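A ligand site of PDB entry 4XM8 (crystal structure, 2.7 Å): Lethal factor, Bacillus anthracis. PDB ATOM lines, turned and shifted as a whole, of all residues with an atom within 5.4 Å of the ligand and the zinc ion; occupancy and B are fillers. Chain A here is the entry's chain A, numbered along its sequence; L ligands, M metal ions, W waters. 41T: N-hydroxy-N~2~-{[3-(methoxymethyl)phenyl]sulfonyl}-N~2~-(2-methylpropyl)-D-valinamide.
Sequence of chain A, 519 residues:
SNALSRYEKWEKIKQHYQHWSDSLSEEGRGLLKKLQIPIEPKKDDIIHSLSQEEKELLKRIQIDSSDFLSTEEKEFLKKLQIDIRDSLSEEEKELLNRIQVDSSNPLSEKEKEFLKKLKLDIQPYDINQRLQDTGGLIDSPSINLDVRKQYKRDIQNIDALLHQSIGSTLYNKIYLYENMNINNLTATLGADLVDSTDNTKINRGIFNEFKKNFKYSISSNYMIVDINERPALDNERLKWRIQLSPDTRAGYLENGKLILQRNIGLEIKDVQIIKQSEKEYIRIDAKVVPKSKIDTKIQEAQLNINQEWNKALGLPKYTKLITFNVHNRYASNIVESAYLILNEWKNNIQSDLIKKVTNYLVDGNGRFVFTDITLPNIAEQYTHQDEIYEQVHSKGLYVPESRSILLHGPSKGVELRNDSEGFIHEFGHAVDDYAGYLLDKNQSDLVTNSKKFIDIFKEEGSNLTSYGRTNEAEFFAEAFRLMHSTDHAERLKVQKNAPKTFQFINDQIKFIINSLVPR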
ATOM      1  N   THR A 188      -3.559  -8.907  15.048  1.00  0.00           N
ATOM      2  CA  THR A 188      -2.586  -8.170  15.840  1.00  0.00           C
ATOM      3  C   THR A 188      -2.575  -6.693  15.466  1.00  0.00           C
ATOM      4  O   THR A 188      -2.624  -5.822  16.341  1.00  0.00           O
ATOM      5  CB  THR A 188      -1.167  -8.755  15.670  1.00  0.00           C
ATOM      6  N   VAL A 392      -3.983 -28.615  19.106  1.00  0.00           N
ATOM      7  CA  VAL A 392      -4.156 -27.268  19.618  1.00  0.00           C
ATOM      8  C   VAL A 392      -4.015 -26.224  18.523  1.00  0.00           C
ATOM      9  O   VAL A 392      -3.094 -26.292  17.711  1.00  0.00           O
ATOM     10  CB  VAL A 392      -3.150 -26.957  20.744  1.00  0.00           C
ATOM     11  CG1 VAL A 392      -3.389 -25.576  21.309  1.00  0.00           C
ATOM     12  CG2 VAL A 392      -3.226 -28.003  21.848  1.00  0.00           C
ATOM     13  N   SER A 394      -3.513 -22.070  18.340  1.00  0.00           N
ATOM     14  CA  SER A 394      -3.199 -20.886  19.117  1.00  0.00           C
ATOM     15  C   SER A 394      -2.248 -20.042  18.297  1.00  0.00           C
ATOM     16  O   SER A 394      -1.967 -20.370  17.148  1.00  0.00           O
ATOM     17  CB  SER A 394      -2.586 -21.252  20.475  1.00  0.00           C
ATOM     18  OG  SER A 394      -1.396 -21.994  20.322  1.00  0.00           O
ATOM     19  N   LYS A 395      -1.740 -18.957  18.871  1.00  0.00           N
ATOM     20  CA  LYS A 395      -0.841 -18.089  18.138  1.00  0.00           C
ATOM     21  C   LYS A 395       0.518 -18.741  17.978  1.00  0.00           C
ATOM     22  O   LYS A 395       1.164 -18.624  16.945  1.00  0.00           O
ATOM     23  CB  LYS A 395      -0.707 -16.731  18.834  1.00  0.00           C
ATOM     24  CG  LYS A 395       0.153 -15.730  18.082  1.00  0.00           C
ATOM     25  CD  LYS A 395      -0.675 -14.586  17.562  1.00  0.00           C
ATOM     26  CE  LYS A 395       0.149 -13.669  16.671  1.00  0.00           C
ATOM     27  NZ  LYS A 395       0.684 -14.372  15.480  1.00  0.00           N
ATOM     28  N   GLY A 396       0.941 -19.445  19.028  1.00  0.00           N
ATOM     29  CA  GLY A 396       2.255 -20.041  19.051  1.00  0.00           C
ATOM     30  C   GLY A 396       2.270 -21.353  19.821  1.00  0.00           C
ATOM     31  O   GLY A 396       1.357 -21.650  20.583  1.00  0.00           O
ATOM     32  N   LEU A 397       3.321 -22.135  19.616  1.00  0.00           N
ATOM     33  CA  LEU A 397       3.411 -23.454  20.213  1.00  0.00           C
ATOM     34  C   LEU A 397       4.847 -23.964  20.175  1.00  0.00           C
ATOM     35  O   LEU A 397       5.605 -23.618  19.275  1.00  0.00           O
ATOM     36  CB  LEU A 397       2.482 -24.424  19.498  1.00  0.00           C
ATOM     37  CG  LEU A 397       1.839 -25.551  20.307  1.00  0.00           C
ATOM     38  CD1 LEU A 397       0.840 -24.984  21.293  1.00  0.00           C
ATOM     39  CD2 LEU A 397       1.181 -26.567  19.383  1.00  0.00           C
ATOM     40  N   TYR A 398       5.210 -24.766  21.158  1.00  0.00           N
ATOM     41  CA  TYR A 398       6.458 -25.528  21.083  1.00  0.00           C
ATOM     42  C   TYR A 398       6.154 -27.012  21.171  1.00  0.00           C
ATOM     43  O   TYR A 398       5.490 -27.475  22.104  1.00  0.00           O
ATOM     44  CB  TYR A 398       7.433 -25.125  22.183  1.00  0.00           C
ATOM     45  CG  TYR A 398       8.692 -25.967  22.138  1.00  0.00           C
ATOM     46  CD1 TYR A 398       9.646 -25.765  21.150  1.00  0.00           C
ATOM     47  CD2 TYR A 398       8.907 -26.975  23.073  1.00  0.00           C
ATOM     48  CE1 TYR A 398      10.785 -26.531  21.098  1.00  0.00           C
ATOM     49  CE2 TYR A 398      10.039 -27.757  23.019  1.00  0.00           C
ATOM     50  CZ  TYR A 398      10.979 -27.529  22.036  1.00  0.00           C
ATOM     51  OH  TYR A 398      12.121 -28.301  21.969  1.00  0.00           O
ATOM     52  N   LEU A 407       4.504 -20.648  14.820  1.00  0.00           N
ATOM     53  CA  LEU A 407       3.925 -19.336  15.052  1.00  0.00           C
ATOM     54  C   LEU A 407       2.867 -19.003  14.013  1.00  0.00           C
ATOM     55  O   LEU A 407       3.156 -18.939  12.815  1.00  0.00           O
ATOM     56  CB  LEU A 407       5.004 -18.260  15.039  1.00  0.00           C
ATOM     57  CG  LEU A 407       4.649 -17.007  15.831  1.00  0.00           C
ATOM     58  CD1 LEU A 407       4.650 -17.317  17.313  1.00  0.00           C
ATOM     59  CD2 LEU A 407       5.611 -15.876  15.513  1.00  0.00           C
ATOM     60  N   LYS A 412      -4.990 -13.564  17.069  1.00  0.00           N
ATOM     61  CA  LYS A 412      -4.656 -12.675  18.180  1.00  0.00           C
ATOM     62  C   LYS A 412      -4.180 -13.493  19.373  1.00  0.00           C
ATOM     63  O   LYS A 412      -4.763 -14.539  19.694  1.00  0.00           O
ATOM     64  CB  LYS A 412      -5.854 -11.811  18.574  1.00  0.00           C
ATOM     65  N   GLY A 413      -3.137 -13.027  20.039  1.00  0.00           N
ATOM     66  CA  GLY A 413      -2.557 -13.772  21.134  1.00  0.00           C
ATOM     67  C   GLY A 413      -3.021 -13.308  22.505  1.00  0.00           C
ATOM     68  O   GLY A 413      -3.422 -12.167  22.689  1.00  0.00           O
ATOM     69  N   VAL A 414      -2.953 -14.219  23.482  1.00  0.00           N
ATOM     70  CA  VAL A 414      -3.375 -13.925  24.838  1.00  0.00           C
ATOM     71  C   VAL A 414      -2.347 -13.081  25.583  1.00  0.00           C
ATOM     72  O   VAL A 414      -1.195 -13.493  25.749  1.00  0.00           O
ATOM     73  CB  VAL A 414      -3.642 -15.219  25.634  1.00  0.00           C
ATOM     74  CG1 VAL A 414      -3.775 -14.912  27.119  1.00  0.00           C
ATOM     75  CG2 VAL A 414      -4.877 -15.927  25.105  1.00  0.00           C
ATOM     76  N   LEU A 416      -0.272 -10.925  25.192  1.00  0.00           N
ATOM     77  CA  LEU A 416       0.981 -10.454  24.628  1.00  0.00           C
ATOM     78  C   LEU A 416       0.750  -9.326  23.626  1.00  0.00           C
ATOM     79  O   LEU A 416      -0.315  -9.220  23.027  1.00  0.00           O
ATOM     80  CB  LEU A 416       1.741 -11.596  23.948  1.00  0.00           C
ATOM     81  CG  LEU A 416       2.166 -12.761  24.842  1.00  0.00           C
ATOM     82  CD1 LEU A 416       3.123 -13.684  24.100  1.00  0.00           C
ATOM     83  CD2 LEU A 416       2.794 -12.230  26.112  1.00  0.00           C
ATOM     84  N   ARG A 417       1.778  -8.487  23.453  1.00  0.00           N
ATOM     85  CA  ARG A 417       1.691  -7.357  22.540  1.00  0.00           C
ATOM     86  C   ARG A 417       1.970  -7.789  21.095  1.00  0.00           C
ATOM     87  O   ARG A 417       1.048  -7.911  20.285  1.00  0.00           O
ATOM     88  CB  ARG A 417       2.670  -6.255  22.948  1.00  0.00           C
ATOM     89  N   ASN A 418       3.245  -8.010  20.791  1.00  0.00           N
ATOM     90  CA  ASN A 418       3.645  -8.398  19.444  1.00  0.00           C
ATOM     91  C   ASN A 418       4.051  -9.865  19.361  1.00  0.00           C
ATOM     92  O   ASN A 418       4.053 -10.576  20.366  1.00  0.00           O
ATOM     93  CB  ASN A 418       4.788  -7.505  18.953  1.00  0.00           C
ATOM     94  CG  ASN A 418       5.955  -7.469  19.924  1.00  0.00           C
ATOM     95  OD1 ASN A 418       6.449  -8.510  20.365  1.00  0.00           O
ATOM     96  ND2 ASN A 418       6.408  -6.265  20.269  1.00  0.00           N
ATOM     97  N   ASP A 419       4.394 -10.311  18.161  1.00  0.00           N
ATOM     98  CA  ASP A 419       4.773 -11.697  17.935  1.00  0.00           C
ATOM     99  C   ASP A 419       6.202 -11.963  18.401  1.00  0.00           C
ATOM    100  O   ASP A 419       6.576 -13.110  18.649  1.00  0.00           O
ATOM    101  CB  ASP A 419       4.629 -12.070  16.456  1.00  0.00           C
ATOM    102  CG  ASP A 419       3.245 -11.753  15.915  1.00  0.00           C
ATOM    103  OD1 ASP A 419       2.378 -11.331  16.703  1.00  0.00           O
ATOM    104  OD2 ASP A 419       3.027 -11.953  14.697  1.00  0.00           O
ATOM    105  N   GLY A 422       6.101 -13.299  21.637  1.00  0.00           N
ATOM    106  CA  GLY A 422       5.532 -14.631  21.519  1.00  0.00           C
ATOM    107  C   GLY A 422       6.581 -15.680  21.202  1.00  0.00           C
ATOM    108  O   GLY A 422       6.597 -16.753  21.807  1.00  0.00           O
ATOM    109  N   PHE A 423       7.466 -15.363  20.259  1.00  0.00           N
ATOM    110  CA  PHE A 423       8.507 -16.295  19.853  1.00  0.00           C
ATOM    111  C   PHE A 423       9.471 -16.584  20.999  1.00  0.00           C
ATOM    112  O   PHE A 423       9.794 -17.740  21.272  1.00  0.00           O
ATOM    113  CB  PHE A 423       9.291 -15.742  18.659  1.00  0.00           C
ATOM    114  CG  PHE A 423      10.339 -16.670  18.131  1.00  0.00           C
ATOM    115  CD1 PHE A 423       9.995 -17.691  17.259  1.00  0.00           C
ATOM    116  CD2 PHE A 423      11.668 -16.536  18.507  1.00  0.00           C
ATOM    117  CE1 PHE A 423      10.955 -18.558  16.769  1.00  0.00           C
ATOM    118  CE2 PHE A 423      12.630 -17.392  18.026  1.00  0.00           C
ATOM    119  CZ  PHE A 423      12.275 -18.406  17.149  1.00  0.00           C
ATOM    120  N   HIS A 425       8.922 -16.373  24.090  1.00  0.00           N
ATOM    121  CA  HIS A 425       8.178 -17.231  25.012  1.00  0.00           C
ATOM    122  C   HIS A 425       8.281 -18.686  24.576  1.00  0.00           C
ATOM    123  O   HIS A 425       8.551 -19.573  25.389  1.00  0.00           O
ATOM    124  CB  HIS A 425       6.714 -16.789  25.085  1.00  0.00           C
ATOM    125  CG  HIS A 425       5.810 -17.784  25.749  1.00  0.00           C
ATOM    126  ND1 HIS A 425       5.319 -17.603  27.022  1.00  0.00           N
ATOM    127  CD2 HIS A 425       5.299 -18.954  25.306  1.00  0.00           C
ATOM    128  CE1 HIS A 425       4.546 -18.621  27.334  1.00  0.00           C
ATOM    129  NE2 HIS A 425       4.520 -19.458  26.321  1.00  0.00           N
ATOM    130  N   GLU A 426       8.066 -18.938  23.286  1.00  0.00           N
ATOM    131  CA  GLU A 426       8.183 -20.285  22.743  1.00  0.00           C
ATOM    132  C   GLU A 426       9.593 -20.820  22.883  1.00  0.00           C
ATOM    133  O   GLU A 426       9.811 -22.005  23.138  1.00  0.00           O
ATOM    134  CB  GLU A 426       7.760 -20.325  21.272  1.00  0.00           C
ATOM    135  CG  GLU A 426       6.373 -19.774  20.990  1.00  0.00           C
ATOM    136  CD  GLU A 426       5.272 -20.563  21.650  1.00  0.00           C
ATOM    137  OE1 GLU A 426       4.142 -20.041  21.744  1.00  0.00           O
ATOM    138  OE2 GLU A 426       5.524 -21.705  22.074  1.00  0.00           O
ATOM    139  N   HIS A 429      10.382 -22.357  26.087  1.00  0.00           N
ATOM    140  CA  HIS A 429       9.968 -23.755  26.140  1.00  0.00           C
ATOM    141  C   HIS A 429      11.080 -24.683  25.664  1.00  0.00           C
ATOM    142  O   HIS A 429      11.277 -25.766  26.224  1.00  0.00           O
ATOM    143  CB  HIS A 429       8.715 -23.977  25.299  1.00  0.00           C
ATOM    144  CG  HIS A 429       7.440 -23.751  26.049  1.00  0.00           C
ATOM    145  ND1 HIS A 429       7.304 -24.048  27.385  1.00  0.00           N
ATOM    146  CD2 HIS A 429       6.250 -23.256  25.648  1.00  0.00           C
ATOM    147  CE1 HIS A 429       6.077 -23.749  27.776  1.00  0.00           C
ATOM    148  NE2 HIS A 429       5.418 -23.265  26.741  1.00  0.00           N
ATOM    149  N   TYR A 467      -1.519 -15.884  32.568  1.00  0.00           N
ATOM    150  CA  TYR A 467      -1.380 -17.151  31.849  1.00  0.00           C
ATOM    151  C   TYR A 467      -0.239 -17.976  32.405  1.00  0.00           C
ATOM    152  O   TYR A 467      -0.191 -19.191  32.232  1.00  0.00           O
ATOM    153  CB  TYR A 467      -1.175 -16.911  30.347  1.00  0.00           C
ATOM    154  CG  TYR A 467      -1.193 -18.201  29.559  1.00  0.00           C
ATOM    155  CD1 TYR A 467      -2.390 -18.829  29.254  1.00  0.00           C
ATOM    156  CD2 TYR A 467      -0.017 -18.811  29.161  1.00  0.00           C
ATOM    157  CE1 TYR A 467      -2.415 -20.014  28.554  1.00  0.00           C
ATOM    158  CE2 TYR A 467      -0.031 -20.002  28.466  1.00  0.00           C
ATOM    159  CZ  TYR A 467      -1.235 -20.600  28.160  1.00  0.00           C
ATOM    160  OH  TYR A 467      -1.249 -21.791  27.465  1.00  0.00           O
ATOM    161  N   GLU A 474       4.388 -23.435  31.493  1.00  0.00           N
ATOM    162  CA  GLU A 474       3.921 -22.113  31.093  1.00  0.00           C
ATOM    163  C   GLU A 474       4.525 -21.010  31.955  1.00  0.00           C
ATOM    164  O   GLU A 474       4.931 -19.964  31.448  1.00  0.00           O
ATOM    165  CB  GLU A 474       2.394 -22.036  31.159  1.00  0.00           C
ATOM    166  CG  GLU A 474       1.682 -23.056  30.289  1.00  0.00           C
ATOM    167  CD  GLU A 474       1.945 -22.836  28.808  1.00  0.00           C
ATOM    168  OE1 GLU A 474       2.465 -21.762  28.468  1.00  0.00           O
ATOM    169  OE2 GLU A 474       1.628 -23.740  28.002  1.00  0.00           O
ATOM    170  N   ALA A 477       8.052 -20.396  30.924  1.00  0.00           N
ATOM    171  CA  ALA A 477       8.117 -19.709  29.630  1.00  0.00           C
ATOM    172  C   ALA A 477       7.819 -18.219  29.772  1.00  0.00           C
ATOM    173  O   ALA A 477       8.541 -17.379  29.236  1.00  0.00           O
ATOM    174  CB  ALA A 477       7.165 -20.351  28.643  1.00  0.00           C
ATOM    175  N   GLU A 478       6.757 -17.899  30.496  1.00  0.00           N
ATOM    176  CA  GLU A 478       6.414 -16.504  30.771  1.00  0.00           C
ATOM    177  C   GLU A 478       7.522 -15.797  31.554  1.00  0.00           C
ATOM    178  O   GLU A 478       7.879 -14.656  31.251  1.00  0.00           O
ATOM    179  CB  GLU A 478       5.094 -16.408  31.533  1.00  0.00           C
ATOM    180  CG  GLU A 478       3.868 -16.694  30.687  1.00  0.00           C
ATOM    181  CD  GLU A 478       3.601 -15.603  29.662  1.00  0.00           C
ATOM    182  OE1 GLU A 478       2.699 -14.772  29.905  1.00  0.00           O
ATOM    183  OE2 GLU A 478       4.292 -15.586  28.617  1.00  0.00           O
HETATM  184  C1  41T L   1       0.301 -20.294  23.846  1.00  0.00           C
HETATM  185  C2  41T L   1       1.573 -20.792  24.483  1.00  0.00           C
HETATM  186  O5  41T L   1       3.732 -21.721  24.201  1.00  0.00           O
HETATM  187  N6  41T L   1       0.027 -18.850  23.993  1.00  0.00           N
HETATM  188  C7  41T L   1       0.231 -18.305  25.343  1.00  0.00           C
HETATM  189  C8  41T L   1       1.034 -17.008  25.271  1.00  0.00           C
HETATM  190  C9  41T L   1       2.485 -17.259  24.891  1.00  0.00           C
HETATM  191  C10 41T L   1       0.955 -16.214  26.574  1.00  0.00           C
HETATM  192  C14 41T L   1       0.587 -17.134  22.053  1.00  0.00           C
HETATM  193  C15 41T L   1       0.346 -15.770  21.934  1.00  0.00           C
HETATM  194  C16 41T L   1       1.257 -14.953  21.265  1.00  0.00           C
HETATM  195  C19 41T L   1       1.730 -17.698  21.500  1.00  0.00           C
HETATM  196  C20 41T L   1       0.966 -13.478  21.145  1.00  0.00           C
HETATM  197  C22 41T L   1       0.664 -11.702  19.630  1.00  0.00           C
HETATM  198  C24 41T L   1      -0.689 -22.568  24.245  1.00  0.00           C
HETATM  199  O3  41T L   1       1.674 -20.930  25.939  1.00  0.00           O
HETATM  200  N4  41T L   1       2.624 -21.139  23.691  1.00  0.00           N
HETATM  201  S11 41T L   1      -0.499 -18.027  22.819  1.00  0.00           S
HETATM  202  O12 41T L   1      -1.522 -17.145  23.295  1.00  0.00           O
HETATM  203  O13 41T L   1      -1.069 -18.908  21.851  1.00  0.00           O
HETATM  204  C17 41T L   1       2.400 -15.517  20.712  1.00  0.00           C
HETATM  205  C18 41T L   1       2.640 -16.881  20.831  1.00  0.00           C
HETATM  206  O21 41T L   1       1.217 -13.008  19.825  1.00  0.00           O
HETATM  207  C23 41T L   1      -0.827 -21.077  24.517  1.00  0.00           C
HETATM  208  C25 41T L   1      -2.254 -20.617  24.188  1.00  0.00           C
HETATM  209 ZN    ZN M   1       3.519 -21.774  26.255  1.00  0.00          ZN
HETATM  210  O   HOH W   1       3.634 -24.613  23.708  1.00  0.00           O
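OE1 of Glu 426 is in hydrogen-bond range of N4 of the ligand (2.7 Å). The backbone NH (N) of Lys 395 is in hydrogen-bond range of an oxygen (O13) of the ligand (3.1 Å). An oxygen (O3) of the ligand lies close to the side-chain hydroxyl of Tyr 467. O13 of the ligand lies close to OG of Ser 394 (3.5 Å). O of Gly 396 lies within hydrogen-bond range of N4 of the ligand. The backbone NH of Val 414 sits at hydrogen-bond distance from an oxygen (O12) of the ligand (3.3 Å).
ND1 of His 425 is in hydrogen-bond range of OE2 of Glu 478 (2.8 Å). The side-chain carboxylate of Glu 426 is in hydrogen-bond range of the backbone NH of Leu 397, 3.1 Å away. The backbone NH (N) of Tyr 398 sits at hydrogen-bond distance from the side-chain carboxylate (OE2) of Glu 426, 3.2 Å away. The side-chain amino group of Lys 395 lies within salt-bridge range of the side-chain carboxylate of Asp 419, 3.5 Å away. The backbone carbonyl oxygen of Gly 396 is in hydrogen-bond range of the side-chain hydroxyl of Ser 394.
Gly 413 touches the ligand. Leu 416 touches the ligand (CB to C20, 3.5 Å). O of Arg 417 touches C22 of the ligand (3.9 Å). Asn 418 touches the ligand. Asp 419 touches the ligand. CA of Gly 422 touches C17 of the ligand, 3.4 Å away. Glu 478 touches the ligand (OE2 to C10, 3.96 Å). Along chain A the residues within 4 Å of the ligand span positions 394 to 478. The nearest printed residue that does not touch the ligand is Leu 407 (4.1 Å).
The zinc ion is bound by an oxygen (O3) of the ligand, an oxygen (O5) of the ligand, the side-chain carboxylate (OE1) of Glu 474, a ring nitrogen (NE2) of His 429 and a ring nitrogen (NE2) of His 425. The zinc ion has five donor atoms within binding distance.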
